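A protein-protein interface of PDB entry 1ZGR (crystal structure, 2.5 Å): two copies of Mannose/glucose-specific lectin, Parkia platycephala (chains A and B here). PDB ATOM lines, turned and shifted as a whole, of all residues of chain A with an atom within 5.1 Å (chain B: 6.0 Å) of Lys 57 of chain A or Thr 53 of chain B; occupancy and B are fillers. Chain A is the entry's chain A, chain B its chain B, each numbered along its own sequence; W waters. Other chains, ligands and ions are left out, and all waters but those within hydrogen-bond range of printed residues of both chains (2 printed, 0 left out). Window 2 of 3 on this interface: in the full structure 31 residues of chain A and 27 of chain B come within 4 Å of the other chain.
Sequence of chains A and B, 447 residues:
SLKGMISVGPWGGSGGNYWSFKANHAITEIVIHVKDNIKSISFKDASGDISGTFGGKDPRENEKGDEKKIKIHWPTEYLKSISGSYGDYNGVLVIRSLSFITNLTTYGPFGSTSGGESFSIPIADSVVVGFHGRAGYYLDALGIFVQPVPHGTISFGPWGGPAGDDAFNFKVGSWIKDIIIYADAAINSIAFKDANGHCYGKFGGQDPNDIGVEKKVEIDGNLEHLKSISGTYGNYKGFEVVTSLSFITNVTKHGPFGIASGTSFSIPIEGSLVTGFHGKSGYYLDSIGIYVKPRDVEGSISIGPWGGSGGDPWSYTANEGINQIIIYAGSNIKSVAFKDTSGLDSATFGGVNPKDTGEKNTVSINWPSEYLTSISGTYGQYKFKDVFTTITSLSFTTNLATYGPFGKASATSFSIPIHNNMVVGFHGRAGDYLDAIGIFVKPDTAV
The side-chain amino group of Lys 57 of chain A is in hydrogen-bond range of the side-chain hydroxyl of Thr 53 of chain B (3.3 Å). N of Thr 53 of chain B lies within hydrogen-bond range of O of Thr 53 of chain A.
N of Phe 54 of chain B is in hydrogen-bond range of O of Ile 41 of chain B. The backbone carbonyl oxygen (O) of Tyr 137 of chain A is in hydrogen-bond range of the backbone NH (N) of Lys 57 of chain A (3.3 Å).
CA of Gly 52 of chain A touches O of Thr 53 of chain B (3.3 Å). CA of Gly 52 of chain A touches CD2 of Phe 54 of chain B (3.5 Å). Thr 53 of chain A touches Gly 52 of chain B (O to CA, 3.3 Å). Ser 51 of chain B touches Phe 54 of chain A. Gly 52 of chain B touches Phe 54 of chain A (CA to CD2, 3.6 Å).
Ser 42 of chain B touches none of the printed residues of chain A. Of the printed residues of chain A, Gly 52 of chain B touches Thr 53 and Phe 54. Thr 53 of chain B touches just these residues of chain A: Gly 52 (3.3 Å), Thr 53 (2.9 Å) and Lys 57 (3.3 Å). Of the printed residues of chain A, Phe 54 of chain B touches Gly 52. The nearest residue of chain B that does not touch Lys 57 of chain A is Ser 42 of chain B (4.2 Å). The nearest printed residue of chain B that does not touch Gly 52 of chain A is Gly 52 of chain B (4.6 Å).
Hydrophobic or aromatic side chains of chain B within 4 Å of the printed part of chain A: Phe 54. Of the 9 printed residues of chain A, 4 touch a printed residue of chain B.
Gly 52 of chain A touches Thr 53 of chain B, and with the chains exchanged Thr 53 of chain A touches Gly 52 of chain B. Gly 52 of chain A touches Phe 54 of chain B, and with the chains exchanged Phe 54 of chain A touches Gly 52 of chain B. Thr 53 of chain B touches its own counterpart, Thr 53 of chain A. 5 positions are printed for both chains. Of the 7 pairs that touch across the chains among the printed residues, 5 have their exchanged pair printed and touching as well.
Water W2 lies within hydrogen-bond range of the side-chain hydroxyl of Ser 42 of chain B (2.9 Å), the side-chain hydroxyl of Thr 53 of chain B (2.9 Å) and the side-chain amino group of Lys 57 of chain A (3.2 Å). Water W1 lies within hydrogen-bond range of the backbone NH (N) of Gly 52 of chain B, the side-chain amino group (NZ) of Lys 57 of chain A and the side-chain hydroxyl (OG) of Ser 42 of chain B.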
ATOM      1  N   GLY A  52      12.202  12.749 -17.402  1.00  0.00           N
ATOM      2  CA  GLY A  52      11.687  12.300 -18.710  1.00  0.00           C
ATOM      3  C   GLY A  52      12.052  10.838 -18.957  1.00  0.00           C
ATOM      4  O   GLY A  52      12.971  10.288 -18.324  1.00  0.00           O
ATOM      5  N   THR A  53      11.305  10.204 -19.851  1.00  0.00           N
ATOM      6  CA  THR A  53      11.330   8.757 -20.023  1.00  0.00           C
ATOM      7  C   THR A  53      12.244   8.365 -21.153  1.00  0.00           C
ATOM      8  O   THR A  53      12.144   8.919 -22.256  1.00  0.00           O
ATOM      9  CB  THR A  53       9.936   8.283 -20.359  1.00  0.00           C
ATOM     10  OG1 THR A  53       9.089   8.567 -19.251  1.00  0.00           O
ATOM     11  CG2 THR A  53       9.882   6.729 -20.487  1.00  0.00           C
ATOM     12  N   PHE A  54      13.129   7.413 -20.878  1.00  0.00           N
ATOM     13  CA  PHE A  54      14.047   6.936 -21.901  1.00  0.00           C
ATOM     14  C   PHE A  54      13.606   5.527 -22.307  1.00  0.00           C
ATOM     15  O   PHE A  54      13.470   4.620 -21.449  1.00  0.00           O
ATOM     16  CB  PHE A  54      15.502   6.981 -21.421  1.00  0.00           C
ATOM     17  CG  PHE A  54      15.910   8.313 -20.793  1.00  0.00           C
ATOM     18  CD1 PHE A  54      15.932   8.463 -19.410  1.00  0.00           C
ATOM     19  CD2 PHE A  54      16.280   9.407 -21.587  1.00  0.00           C
ATOM     20  CE1 PHE A  54      16.303   9.705 -18.811  1.00  0.00           C
ATOM     21  CE2 PHE A  54      16.664  10.663 -21.007  1.00  0.00           C
ATOM     22  CZ  PHE A  54      16.673  10.808 -19.615  1.00  0.00           C
ATOM     23  N   GLY A  55      13.382   5.355 -23.610  1.00  0.00           N
ATOM     24  CA  GLY A  55      12.815   4.135 -24.159  1.00  0.00           C
ATOM     25  C   GLY A  55      11.305   4.114 -24.004  1.00  0.00           C
ATOM     26  O   GLY A  55      10.698   5.089 -23.565  1.00  0.00           O
ATOM     27  N   GLY A  56      10.704   2.981 -24.353  1.00  0.00           N
ATOM     28  CA  GLY A  56       9.249   2.821 -24.326  1.00  0.00           C
ATOM     29  C   GLY A  56       8.533   3.418 -25.527  1.00  0.00           C
ATOM     30  O   GLY A  56       7.422   3.916 -25.392  1.00  0.00           O
ATOM     31  N   LYS A  57       9.131   3.324 -26.712  1.00  0.00           N
ATOM     32  CA  LYS A  57       8.682   4.169 -27.845  1.00  0.00           C
ATOM     33  C   LYS A  57       7.866   3.565 -28.996  1.00  0.00           C
ATOM     34  O   LYS A  57       7.526   4.311 -29.915  1.00  0.00           O
ATOM     35  CB  LYS A  57       9.880   4.936 -28.436  1.00  0.00           C
ATOM     36  CG  LYS A  57      10.726   5.641 -27.370  1.00  0.00           C
ATOM     37  CD  LYS A  57      10.437   7.130 -27.281  1.00  0.00           C
ATOM     38  CE  LYS A  57      11.445   7.904 -28.127  1.00  0.00           C
ATOM     39  NZ  LYS A  57      11.284   9.361 -27.856  1.00  0.00           N
ATOM     40  N   ASP A  58       7.523   2.272 -28.969  1.00  0.00           N
ATOM     41  CA  ASP A  58       6.801   1.642 -30.123  1.00  0.00           C
ATOM     42  C   ASP A  58       5.452   2.297 -30.439  1.00  0.00           C
ATOM     43  O   ASP A  58       4.559   2.348 -29.581  1.00  0.00           O
ATOM     44  CB  ASP A  58       6.589   0.130 -29.936  1.00  0.00           C
ATOM     45  CG  ASP A  58       7.642  -0.508 -29.060  1.00  0.00           C
ATOM     46  OD1 ASP A  58       7.874  -1.736 -29.193  1.00  0.00           O
ATOM     47  OD2 ASP A  58       8.285   0.145 -28.200  1.00  0.00           O
ATOM     48  N   GLY A 136      15.841   3.952 -27.704  1.00  0.00           N
ATOM     49  CA  GLY A 136      15.078   4.203 -28.943  1.00  0.00           C
ATOM     50  C   GLY A 136      13.718   3.640 -28.585  1.00  0.00           C
ATOM     51  O   GLY A 136      13.071   4.135 -27.657  1.00  0.00           O
ATOM     52  N   TYR A 137      13.322   2.559 -29.251  1.00  0.00           N
ATOM     53  CA  TYR A 137      12.153   1.771 -28.857  1.00  0.00           C
ATOM     54  C   TYR A 137      12.328   1.139 -27.490  1.00  0.00           C
ATOM     55  O   TYR A 137      11.350   0.943 -26.766  1.00  0.00           O
ATOM     56  CB  TYR A 137      11.880   0.651 -29.869  1.00  0.00           C
ATOM     57  CG  TYR A 137      11.236   1.099 -31.162  1.00  0.00           C
ATOM     58  CD1 TYR A 137      11.205   2.454 -31.523  1.00  0.00           C
ATOM     59  CD2 TYR A 137      10.680   0.157 -32.050  1.00  0.00           C
ATOM     60  CE1 TYR A 137      10.627   2.867 -32.728  1.00  0.00           C
ATOM     61  CE2 TYR A 137      10.100   0.563 -33.265  1.00  0.00           C
ATOM     62  CZ  TYR A 137      10.086   1.921 -33.594  1.00  0.00           C
ATOM     63  OH  TYR A 137       9.528   2.357 -34.773  1.00  0.00           O
ATOM     64  N   VAL B  31      10.296  16.596 -31.067  1.00  0.00           N
ATOM     65  CA  VAL B  31       9.265  15.614 -31.340  1.00  0.00           C
ATOM     66  C   VAL B  31       8.087  15.850 -30.411  1.00  0.00           C
ATOM     67  O   VAL B  31       8.227  15.787 -29.218  1.00  0.00           O
ATOM     68  CB  VAL B  31       9.791  14.166 -31.135  1.00  0.00           C
ATOM     69  CG1 VAL B  31       8.709  13.135 -31.503  1.00  0.00           C
ATOM     70  CG2 VAL B  31      11.082  13.916 -31.920  1.00  0.00           C
ATOM     71  N   SER B  40       2.992  15.380 -25.317  1.00  0.00           N
ATOM     72  CA  SER B  40       4.384  15.137 -24.941  1.00  0.00           C
ATOM     73  C   SER B  40       5.393  15.799 -25.894  1.00  0.00           C
ATOM     74  O   SER B  40       5.052  16.223 -27.005  1.00  0.00           O
ATOM     75  CB  SER B  40       4.640  13.635 -24.879  1.00  0.00           C
ATOM     76  OG  SER B  40       4.777  13.120 -26.188  1.00  0.00           O
ATOM     77  N   ILE B  41       6.637  15.896 -25.431  1.00  0.00           N
ATOM     78  CA  ILE B  41       7.708  16.535 -26.176  1.00  0.00           C
ATOM     79  C   ILE B  41       9.043  15.848 -25.790  1.00  0.00           C
ATOM     80  O   ILE B  41       9.204  15.345 -24.660  1.00  0.00           O
ATOM     81  CB  ILE B  41       7.737  18.060 -25.858  1.00  0.00           C
ATOM     82  CG1 ILE B  41       8.506  18.856 -26.924  1.00  0.00           C
ATOM     83  CG2 ILE B  41       8.294  18.334 -24.437  1.00  0.00           C
ATOM     84  CD1 ILE B  41       8.227  20.358 -26.892  1.00  0.00           C
ATOM     85  N   SER B  42       9.967  15.822 -26.748  1.00  0.00           N
ATOM     86  CA  SER B  42      11.338  15.425 -26.533  1.00  0.00           C
ATOM     87  C   SER B  42      12.220  16.144 -27.550  1.00  0.00           C
ATOM     88  O   SER B  42      11.709  16.787 -28.469  1.00  0.00           O
ATOM     89  CB  SER B  42      11.498  13.914 -26.658  1.00  0.00           C
ATOM     90  OG  SER B  42      11.630  13.512 -28.007  1.00  0.00           O
ATOM     91  N   ILE B  50      19.652  12.294 -27.348  1.00  0.00           N
ATOM     92  CA  ILE B  50      18.251  12.590 -27.063  1.00  0.00           C
ATOM     93  C   ILE B  50      17.998  13.024 -25.621  1.00  0.00           C
ATOM     94  O   ILE B  50      18.759  12.694 -24.704  1.00  0.00           O
ATOM     95  CB  ILE B  50      17.291  11.421 -27.463  1.00  0.00           C
ATOM     96  CG1 ILE B  50      17.640  10.126 -26.723  1.00  0.00           C
ATOM     97  CG2 ILE B  50      17.194  11.288 -29.010  1.00  0.00           C
ATOM     98  CD1 ILE B  50      16.566   9.026 -26.861  1.00  0.00           C
ATOM     99  N   SER B  51      16.901  13.758 -25.441  1.00  0.00           N
ATOM    100  CA  SER B  51      16.433  14.190 -24.134  1.00  0.00           C
ATOM    101  C   SER B  51      15.573  13.163 -23.419  1.00  0.00           C
ATOM    102  O   SER B  51      15.365  13.252 -22.189  1.00  0.00           O
ATOM    103  CB  SER B  51      15.618  15.477 -24.272  1.00  0.00           C
ATOM    104  OG  SER B  51      14.291  15.214 -24.745  1.00  0.00           O
ATOM    105  N   GLY B  52      14.987  12.216 -24.125  1.00  0.00           N
ATOM    106  CA  GLY B  52      13.924  11.470 -23.394  1.00  0.00           C
ATOM    107  C   GLY B  52      12.618  12.282 -23.312  1.00  0.00           C
ATOM    108  O   GLY B  52      12.607  13.517 -23.507  1.00  0.00           O
ATOM    109  N   THR B  53      11.517  11.585 -23.053  1.00  0.00           N
ATOM    110  CA  THR B  53      10.185  12.119 -23.338  1.00  0.00           C
ATOM    111  C   THR B  53       9.513  12.771 -22.127  1.00  0.00           C
ATOM    112  O   THR B  53       9.332  12.154 -21.084  1.00  0.00           O
ATOM    113  CB  THR B  53       9.274  10.982 -23.919  1.00  0.00           C
ATOM    114  OG1 THR B  53       9.762  10.596 -25.208  1.00  0.00           O
ATOM    115  CG2 THR B  53       7.902  11.482 -24.241  1.00  0.00           C
ATOM    116  N   PHE B  54       9.105  14.017 -22.288  1.00  0.00           N
ATOM    117  CA  PHE B  54       8.371  14.695 -21.217  1.00  0.00           C
ATOM    118  C   PHE B  54       6.884  14.730 -21.550  1.00  0.00           C
ATOM    119  O   PHE B  54       6.482  15.257 -22.602  1.00  0.00           O
ATOM    120  CB  PHE B  54       8.977  16.090 -20.952  1.00  0.00           C
ATOM    121  CG  PHE B  54      10.514  16.079 -20.866  1.00  0.00           C
ATOM    122  CD1 PHE B  54      11.299  16.458 -21.975  1.00  0.00           C
ATOM    123  CD2 PHE B  54      11.162  15.661 -19.704  1.00  0.00           C
ATOM    124  CE1 PHE B  54      12.704  16.429 -21.913  1.00  0.00           C
ATOM    125  CE2 PHE B  54      12.566  15.655 -19.611  1.00  0.00           C
ATOM    126  CZ  PHE B  54      13.347  16.044 -20.719  1.00  0.00           C
ATOM    127  N   GLY B  55       6.081  14.161 -20.646  1.00  0.00           N
ATOM    128  CA  GLY B  55       4.656  13.926 -20.884  1.00  0.00           C
ATOM    129  C   GLY B  55       4.353  12.565 -21.504  1.00  0.00           C
ATOM    130  O   GLY B  55       5.236  11.720 -21.693  1.00  0.00           O
ATOM    131  N   GLY B  56       3.085  12.338 -21.805  1.00  0.00           N
ATOM    132  CA  GLY B  56       2.683  11.122 -22.484  1.00  0.00           C
ATOM    133  C   GLY B  56       2.576   9.918 -21.577  1.00  0.00           C
ATOM    134  O   GLY B  56       2.449   8.797 -22.068  1.00  0.00           O
HETATM  135  O   HOH W   1      13.568  11.058 -26.506  1.00  0.00           O
HETATM  136  O   HOH W   2       9.290  11.872 -27.776  1.00  0.00           O
